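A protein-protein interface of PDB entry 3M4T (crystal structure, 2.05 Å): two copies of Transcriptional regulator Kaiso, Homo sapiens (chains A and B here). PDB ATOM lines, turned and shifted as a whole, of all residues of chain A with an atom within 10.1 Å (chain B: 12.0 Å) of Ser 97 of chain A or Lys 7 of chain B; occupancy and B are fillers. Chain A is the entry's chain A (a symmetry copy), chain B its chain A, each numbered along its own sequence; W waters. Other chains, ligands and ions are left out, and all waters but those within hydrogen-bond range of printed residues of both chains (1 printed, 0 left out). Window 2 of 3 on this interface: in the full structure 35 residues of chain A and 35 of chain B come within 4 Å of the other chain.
O of Ser 5 of chain B is in hydrogen-bond range of NZ of Lys 7 of chain B (3.1 Å). The side-chain carboxylate (OD2) of Asp 98 of chain A lies within salt-bridge range of the guanidinium group (NH1) of Arg 96 of chain A (2.8 Å).
Ser 10 of chain B touches Ile 92 of chain A. Val 93 of chain A touches Ile 9 of chain B (C to O, 3.8 Å). Val 93 of chain A touches Ser 10 of chain B (CA to OG, 3.7 Å). Arg 94 of chain A touches Leu 8 of chain B. O of Val 95 of chain A touches O of Lys 7 of chain B, at 3.9 Å. Val 95 of chain A touches Leu 8 of chain B. Arg 96 of chain A touches Lys 7 of chain B (CA to O, 3.6 Å). CG of Arg 96 of chain A touches CD2 of Leu 8 of chain B, at 3.98 Å. Ile 9 of chain B touches Ser 97 of chain A (CD1 to CA, 3.6 Å). Leu 100 of chain A touches Ile 9 of chain B.
O of Lys 7 of chain B sits at hydrogen-bond distance from N of Ser 97 of chain A. The backbone carbonyl oxygen (O) of Ile 9 of chain B is in hydrogen-bond range of the backbone NH (N) of Arg 94 of chain A (3.1 Å). The backbone NH (N) of Ile 9 of chain B lies within hydrogen-bond range of the backbone carbonyl oxygen (O) of Val 95 of chain A (2.7 Å). N of Arg 94 of chain A sits at hydrogen-bond distance from OG of Ser 10 of chain B (2.8 Å). The backbone NH of Ile 92 of chain A lies within hydrogen-bond range of the backbone carbonyl oxygen of Ala 11 of chain B (2.8 Å).
No position is printed for both chains.
Water W1 bridges O of Ile 92 of chain A (3.0 Å) and O of Ala 11 of chain B (3.3 Å).
Of the 16 printed residues of chain A, 7 touch a printed residue of chain B. Printed residues of chain A that touch a printed residue of chain B: Ile 92, Val 93, Arg 94, Val 95, Arg 96, Ser 97 and Leu 100. Hydrophobic or aromatic side chains of chain A that line the printed part of chain B: Ile 92, Val 95 and Leu 100. Printed residues of chain B that touch a printed residue of chain A: Lys 7, Leu 8, Ile 9, Ser 10 and Ala 11. Hydrophobic or aromatic side chains of chain B that line the printed part of chain A: Leu 8 and Ile 9.
Ser 97 of chain A touches two residues of chain B. Lys 7 of chain B touches just these residues of chain A: Val 95, Arg 96 and Ser 97. Of the printed residues of chain B, Val 95 of chain A touches Lys 7, Leu 8 and Ile 9. Of chain B, only Lys 7 and Leu 8 come within 4 Å of Arg 96 of chain A. No residue of chain B comes within 4 Å of Asp 98 of chain A. No residue of chain B comes within 4 Å of Leu 99 of chain A. Leu 100 of chain A touches just one residue of chain B: Ile 9 (3.8 Å). Printed residues of chain A within 4 Å of Leu 8 of chain B: Arg 94 (3.5 Å), Val 95 (3.4 Å) and Arg 96 (3.98 Å). Of the printed residues of chain A, Ala 11 of chain B touches Ile 92. Printed residues of chain B within 4 Å of Val 93 of chain A: Ile 9 and Ser 10. Of the printed residues of chain B, Ile 92 of chain A touches Ser 10 (3.2 Å) and Ala 11 (2.8 Å).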
ATOM      1  N   ARG A  76      -6.804  -0.673 -13.172  1.00  0.00           N
ATOM      2  CA  ARG A  76      -6.173   0.024 -14.297  1.00  0.00           C
ATOM      3  C   ARG A  76      -6.702   1.449 -14.467  1.00  0.00           C
ATOM      4  O   ARG A  76      -7.859   1.733 -14.145  1.00  0.00           O
ATOM      5  CB  ARG A  76      -6.346  -0.807 -15.569  1.00  0.00           C
ATOM      6  CG  ARG A  76      -5.515  -2.128 -15.479  1.00  0.00           C
ATOM      7  CD  ARG A  76      -5.377  -2.792 -16.814  1.00  0.00           C
ATOM      8  NE  ARG A  76      -6.695  -3.134 -17.351  1.00  0.00           N
ATOM      9  CZ  ARG A  76      -7.254  -2.505 -18.377  1.00  0.00           C
ATOM     10  NH1 ARG A  76      -6.602  -1.519 -18.988  1.00  0.00           N
ATOM     11  NH2 ARG A  76      -8.453  -2.869 -18.811  1.00  0.00           N
ATOM     12  N   ILE A  79     -10.041   1.933 -16.296  1.00  0.00           N
ATOM     13  CA  ILE A  79     -11.172   1.482 -15.476  1.00  0.00           C
ATOM     14  C   ILE A  79     -11.499   2.569 -14.460  1.00  0.00           C
ATOM     15  O   ILE A  79     -12.666   2.975 -14.309  1.00  0.00           O
ATOM     16  CB  ILE A  79     -10.867   0.107 -14.781  1.00  0.00           C
ATOM     17  CG1 ILE A  79     -10.578  -0.978 -15.841  1.00  0.00           C
ATOM     18  CG2 ILE A  79     -12.023  -0.316 -13.851  1.00  0.00           C
ATOM     19  CD1 ILE A  79     -11.737  -1.185 -16.917  1.00  0.00           C
ATOM     20  N   ILE A  92     -22.805   4.943 -16.683  1.00  0.00           N
ATOM     21  CA  ILE A  92     -21.699   4.422 -17.501  1.00  0.00           C
ATOM     22  C   ILE A  92     -22.222   4.336 -18.920  1.00  0.00           C
ATOM     23  O   ILE A  92     -23.380   3.966 -19.150  1.00  0.00           O
ATOM     24  CB  ILE A  92     -21.102   3.080 -16.995  1.00  0.00           C
ATOM     25  CG1 ILE A  92     -22.080   1.925 -17.150  1.00  0.00           C
ATOM     26  CG2 ILE A  92     -20.622   3.219 -15.545  1.00  0.00           C
ATOM     27  CD1 ILE A  92     -21.423   0.559 -16.931  1.00  0.00           C
ATOM     28  N   VAL A  93     -21.392   4.749 -19.861  1.00  0.00           N
ATOM     29  CA  VAL A  93     -21.826   4.942 -21.240  1.00  0.00           C
ATOM     30  C   VAL A  93     -20.942   4.131 -22.171  1.00  0.00           C
ATOM     31  O   VAL A  93     -19.723   4.356 -22.238  1.00  0.00           O
ATOM     32  CB  VAL A  93     -21.776   6.453 -21.635  1.00  0.00           C
ATOM     33  CG1 VAL A  93     -21.984   6.650 -23.124  1.00  0.00           C
ATOM     34  CG2 VAL A  93     -22.874   7.223 -20.867  1.00  0.00           C
ATOM     35  N   ARG A  94     -21.553   3.181 -22.870  1.00  0.00           N
ATOM     36  CA  ARG A  94     -20.869   2.400 -23.903  1.00  0.00           C
ATOM     37  C   ARG A  94     -19.501   1.864 -23.429  1.00  0.00           C
ATOM     38  O   ARG A  94     -18.463   2.029 -24.079  1.00  0.00           O
ATOM     39  CB  ARG A  94     -20.732   3.236 -25.175  1.00  0.00           C
ATOM     40  CG  ARG A  94     -22.092   3.695 -25.723  1.00  0.00           C
ATOM     41  CD  ARG A  94     -21.934   4.812 -26.766  1.00  0.00           C
ATOM     42  NE  ARG A  94     -21.848   4.244 -28.108  1.00  0.00           N
ATOM     43  CZ  ARG A  94     -20.717   4.175 -28.799  1.00  0.00           C
ATOM     44  NH1 ARG A  94     -19.595   4.672 -28.275  1.00  0.00           N
ATOM     45  NH2 ARG A  94     -20.701   3.624 -30.002  1.00  0.00           N
ATOM     46  N   VAL A  95     -19.516   1.216 -22.283  1.00  0.00           N
ATOM     47  CA  VAL A  95     -18.339   0.487 -21.787  1.00  0.00           C
ATOM     48  C   VAL A  95     -18.194  -0.843 -22.554  1.00  0.00           C
ATOM     49  O   VAL A  95     -19.158  -1.595 -22.661  1.00  0.00           O
ATOM     50  CB  VAL A  95     -18.535   0.211 -20.277  1.00  0.00           C
ATOM     51  CG1 VAL A  95     -17.492  -0.814 -19.728  1.00  0.00           C
ATOM     52  CG2 VAL A  95     -18.510   1.538 -19.512  1.00  0.00           C
ATOM     53  N   ARG A  96     -16.992  -1.149 -23.057  1.00  0.00           N
ATOM     54  CA  ARG A  96     -16.763  -2.411 -23.759  1.00  0.00           C
ATOM     55  C   ARG A  96     -16.989  -3.548 -22.822  1.00  0.00           C
ATOM     56  O   ARG A  96     -16.558  -3.526 -21.666  1.00  0.00           O
ATOM     57  CB  ARG A  96     -15.340  -2.516 -24.330  1.00  0.00           C
ATOM     58  CG  ARG A  96     -15.009  -1.484 -25.335  1.00  0.00           C
ATOM     59  CD  ARG A  96     -13.502  -1.198 -25.333  1.00  0.00           C
ATOM     60  NE  ARG A  96     -12.808  -2.092 -26.268  1.00  0.00           N
ATOM     61  CZ  ARG A  96     -11.876  -2.991 -25.942  1.00  0.00           C
ATOM     62  NH1 ARG A  96     -11.464  -3.136 -24.682  1.00  0.00           N
ATOM     63  NH2 ARG A  96     -11.345  -3.747 -26.901  1.00  0.00           N
ATOM     64  N   SER A  97     -17.655  -4.565 -23.340  1.00  0.00           N
ATOM     65  CA  SER A  97     -18.060  -5.716 -22.577  1.00  0.00           C
ATOM     66  C   SER A  97     -16.892  -6.464 -21.932  1.00  0.00           C
ATOM     67  O   SER A  97     -17.045  -7.068 -20.861  1.00  0.00           O
ATOM     68  CB  SER A  97     -18.780  -6.689 -23.489  1.00  0.00           C
ATOM     69  OG  SER A  97     -19.410  -7.632 -22.670  1.00  0.00           O
ATOM     70  N   ASP A  98     -15.743  -6.438 -22.589  1.00  0.00           N
ATOM     71  CA  ASP A  98     -14.548  -7.130 -22.042  1.00  0.00           C
ATOM     72  C   ASP A  98     -13.892  -6.387 -20.881  1.00  0.00           C
ATOM     73  O   ASP A  98     -12.956  -6.911 -20.271  1.00  0.00           O
ATOM     74  CB  ASP A  98     -13.515  -7.370 -23.150  1.00  0.00           C
ATOM     75  CG  ASP A  98     -13.087  -6.087 -23.825  1.00  0.00           C
ATOM     76  OD1 ASP A  98     -13.965  -5.252 -24.076  1.00  0.00           O
ATOM     77  OD2 ASP A  98     -11.886  -5.890 -24.111  1.00  0.00           O
ATOM     78  N   LEU A  99     -14.313  -5.142 -20.624  1.00  0.00           N
ATOM     79  CA  LEU A  99     -13.844  -4.398 -19.455  1.00  0.00           C
ATOM     80  C   LEU A  99     -14.832  -4.487 -18.267  1.00  0.00           C
ATOM     81  O   LEU A  99     -14.500  -4.097 -17.140  1.00  0.00           O
ATOM     82  CB  LEU A  99     -13.565  -2.937 -19.823  1.00  0.00           C
ATOM     83  CG  LEU A  99     -12.505  -2.701 -20.914  1.00  0.00           C
ATOM     84  CD1 LEU A  99     -12.353  -1.259 -21.239  1.00  0.00           C
ATOM     85  CD2 LEU A  99     -11.155  -3.289 -20.470  1.00  0.00           C
ATOM     86  N   LEU A 100     -16.013  -5.057 -18.500  1.00  0.00           N
ATOM     87  CA  LEU A 100     -17.079  -5.026 -17.496  1.00  0.00           C
ATOM     88  C   LEU A 100     -16.715  -5.713 -16.195  1.00  0.00           C
ATOM     89  O   LEU A 100     -16.997  -5.172 -15.137  1.00  0.00           O
ATOM     90  CB  LEU A 100     -18.403  -5.599 -18.037  1.00  0.00           C
ATOM     91  CG  LEU A 100     -19.599  -5.492 -17.073  1.00  0.00           C
ATOM     92  CD1 LEU A 100     -19.929  -4.041 -16.737  1.00  0.00           C
ATOM     93  CD2 LEU A 100     -20.866  -6.228 -17.598  1.00  0.00           C
ATOM     94  N   ASP A 101     -16.097  -6.899 -16.244  1.00  0.00           N
ATOM     95  CA  ASP A 101     -15.763  -7.595 -14.974  1.00  0.00           C
ATOM     96  C   ASP A 101     -14.737  -6.798 -14.181  1.00  0.00           C
ATOM     97  O   ASP A 101     -14.839  -6.718 -12.978  1.00  0.00           O
ATOM     98  CB  ASP A 101     -15.245  -9.032 -15.178  1.00  0.00           C
ATOM     99  CG  ASP A 101     -16.305  -9.972 -15.725  1.00  0.00           C
ATOM    100  OD1 ASP A 101     -17.528  -9.664 -15.638  1.00  0.00           O
ATOM    101  OD2 ASP A 101     -15.913 -11.036 -16.260  1.00  0.00           O
ATOM    102  N   GLU A 102     -13.761  -6.210 -14.866  1.00  0.00           N
ATOM    103  CA  GLU A 102     -12.795  -5.307 -14.249  1.00  0.00           C
ATOM    104  C   GLU A 102     -13.467  -4.087 -13.634  1.00  0.00           C
ATOM    105  O   GLU A 102     -13.074  -3.626 -12.563  1.00  0.00           O
ATOM    106  CB  GLU A 102     -11.794  -4.803 -15.280  1.00  0.00           C
ATOM    107  CG  GLU A 102     -10.469  -5.521 -15.283  1.00  0.00           C
ATOM    108  CD  GLU A 102      -9.519  -4.832 -16.203  1.00  0.00           C
ATOM    109  OE1 GLU A 102      -9.698  -4.989 -17.419  1.00  0.00           O
ATOM    110  OE2 GLU A 102      -8.611  -4.117 -15.720  1.00  0.00           O
ATOM    111  N   LEU A 103     -14.441  -3.523 -14.343  1.00  0.00           N
ATOM    112  CA  LEU A 103     -15.194  -2.396 -13.809  1.00  0.00           C
ATOM    113  C   LEU A 103     -15.977  -2.758 -12.530  1.00  0.00           C
ATOM    114  O   LEU A 103     -15.915  -2.041 -11.526  1.00  0.00           O
ATOM    115  CB  LEU A 103     -16.119  -1.784 -14.888  1.00  0.00           C
ATOM    116  CG  LEU A 103     -16.968  -0.577 -14.434  1.00  0.00           C
ATOM    117  CD1 LEU A 103     -16.101   0.630 -14.050  1.00  0.00           C
ATOM    118  CD2 LEU A 103     -18.026  -0.202 -15.503  1.00  0.00           C
ATOM    119  N   ILE A 104     -16.681  -3.885 -12.577  1.00  0.00           N
ATOM    120  CA  ILE A 104     -17.438  -4.377 -11.437  1.00  0.00           C
ATOM    121  C   ILE A 104     -16.484  -4.594 -10.270  1.00  0.00           C
ATOM    122  O   ILE A 104     -16.779  -4.177  -9.140  1.00  0.00           O
ATOM    123  CB  ILE A 104     -18.158  -5.703 -11.798  1.00  0.00           C
ATOM    124  CG1 ILE A 104     -19.308  -5.425 -12.770  1.00  0.00           C
ATOM    125  CG2 ILE A 104     -18.685  -6.435 -10.551  1.00  0.00           C
ATOM    126  CD1 ILE A 104     -19.899  -6.736 -13.365  1.00  0.00           C
ATOM    127  N   LEU A 118     -23.285  -4.315 -10.825  1.00  0.00           N
ATOM    128  CA  LEU A 118     -23.603  -4.446 -12.247  1.00  0.00           C
ATOM    129  C   LEU A 118     -23.664  -5.889 -12.746  1.00  0.00           C
ATOM    130  O   LEU A 118     -24.316  -6.151 -13.760  1.00  0.00           O
ATOM    131  CB  LEU A 118     -22.600  -3.684 -13.116  1.00  0.00           C
ATOM    132  CG  LEU A 118     -22.772  -2.173 -13.231  1.00  0.00           C
ATOM    133  CD1 LEU A 118     -21.605  -1.610 -14.012  1.00  0.00           C
ATOM    134  CD2 LEU A 118     -24.113  -1.851 -13.887  1.00  0.00           C
ATOM    135  N   SER B   5     -19.527  -9.598 -31.584  1.00  0.00           N
ATOM    136  CA  SER B   5     -19.462 -10.197 -30.240  1.00  0.00           C
ATOM    137  C   SER B   5     -19.064  -9.090 -29.292  1.00  0.00           C
ATOM    138  O   SER B   5     -19.260  -9.210 -28.078  1.00  0.00           O
ATOM    139  CB  SER B   5     -18.422 -11.313 -30.208  1.00  0.00           C
ATOM    140  OG  SER B   5     -18.944 -12.443 -29.553  1.00  0.00           O
ATOM    141  N   ARG B   6     -18.497  -8.017 -29.864  1.00  0.00           N
ATOM    142  CA  ARG B   6     -18.062  -6.831 -29.122  1.00  0.00           C
ATOM    143  C   ARG B   6     -19.255  -5.927 -28.774  1.00  0.00           C
ATOM    144  O   ARG B   6     -19.747  -5.134 -29.588  1.00  0.00           O
ATOM    145  CB  ARG B   6     -16.989  -6.071 -29.901  1.00  0.00           C
ATOM    146  CG  ARG B   6     -16.612  -4.700 -29.339  1.00  0.00           C
ATOM    147  CD  ARG B   6     -15.821  -3.856 -30.378  1.00  0.00           C
ATOM    148  NE  ARG B   6     -16.378  -3.930 -31.744  1.00  0.00           N
ATOM    149  CZ  ARG B   6     -17.342  -3.128 -32.209  1.00  0.00           C
ATOM    150  NH1 ARG B   6     -17.867  -2.184 -31.421  1.00  0.00           N
ATOM    151  NH2 ARG B   6     -17.797  -3.268 -33.456  1.00  0.00           N
ATOM    152  N   LYS B   7     -19.678  -6.066 -27.531  1.00  0.00           N
ATOM    153  CA  LYS B   7     -20.840  -5.416 -26.991  1.00  0.00           C
ATOM    154  C   LYS B   7     -20.408  -4.199 -26.207  1.00  0.00           C
ATOM    155  O   LYS B   7     -19.313  -4.188 -25.608  1.00  0.00           O
ATOM    156  CB  LYS B   7     -21.552  -6.391 -26.055  1.00  0.00           C
ATOM    157  CG  LYS B   7     -21.947  -7.727 -26.713  1.00  0.00           C
ATOM    158  CD  LYS B   7     -22.680  -8.651 -25.710  1.00  0.00           C
ATOM    159  CE  LYS B   7     -21.717  -9.347 -24.726  1.00  0.00           C
ATOM    160  NZ  LYS B   7     -20.680 -10.100 -25.489  1.00  0.00           N
ATOM    161  N   LEU B   8     -21.269  -3.184 -26.194  1.00  0.00           N
ATOM    162  CA  LEU B   8     -21.041  -1.982 -25.408  1.00  0.00           C
ATOM    163  C   LEU B   8     -22.155  -1.947 -24.374  1.00  0.00           C
ATOM    164  O   LEU B   8     -23.304  -2.266 -24.705  1.00  0.00           O
ATOM    165  CB  LEU B   8     -21.060  -0.718 -26.289  1.00  0.00           C
ATOM    166  CG  LEU B   8     -20.014  -0.670 -27.421  1.00  0.00           C
ATOM    167  CD1 LEU B   8     -20.278   0.500 -28.422  1.00  0.00           C
ATOM    168  CD2 LEU B   8     -18.554  -0.635 -26.926  1.00  0.00           C
ATOM    169  N   ILE B   9     -21.830  -1.576 -23.139  1.00  0.00           N
ATOM    170  CA  ILE B   9     -22.812  -1.567 -22.067  1.00  0.00           C
ATOM    171  C   ILE B   9     -22.992  -0.157 -21.514  1.00  0.00           C
ATOM    172  O   ILE B   9     -22.010   0.558 -21.286  1.00  0.00           O
ATOM    173  CB  ILE B   9     -22.408  -2.554 -20.959  1.00  0.00           C
ATOM    174  CG1 ILE B   9     -22.372  -3.965 -21.540  1.00  0.00           C
ATOM    175  CG2 ILE B   9     -23.385  -2.511 -19.776  1.00  0.00           C
ATOM    176  CD1 ILE B   9     -21.196  -4.736 -21.115  1.00  0.00           C
ATOM    177  N   SER B  10     -24.252   0.249 -21.385  1.00  0.00           N
ATOM    178  CA  SER B  10     -24.621   1.506 -20.764  1.00  0.00           C
ATOM    179  C   SER B  10     -25.580   1.219 -19.613  1.00  0.00           C
ATOM    180  O   SER B  10     -26.387   0.267 -19.693  1.00  0.00           O
ATOM    181  CB  SER B  10     -25.287   2.391 -21.811  1.00  0.00           C
ATOM    182  OG  SER B  10     -24.338   2.730 -22.807  1.00  0.00           O
ATOM    183  N   ALA B  11     -25.514   2.037 -18.557  1.00  0.00           N
ATOM    184  CA  ALA B  11     -26.417   1.916 -17.407  1.00  0.00           C
ATOM    185  C   ALA B  11     -26.442   3.236 -16.662  1.00  0.00           C
ATOM    186  O   ALA B  11     -25.414   3.911 -16.583  1.00  0.00           O
ATOM    187  CB  ALA B  11     -25.935   0.788 -16.488  1.00  0.00           C
HETATM  188  O   HOH W   1     -26.093   5.239 -19.471  1.00  0.00           O
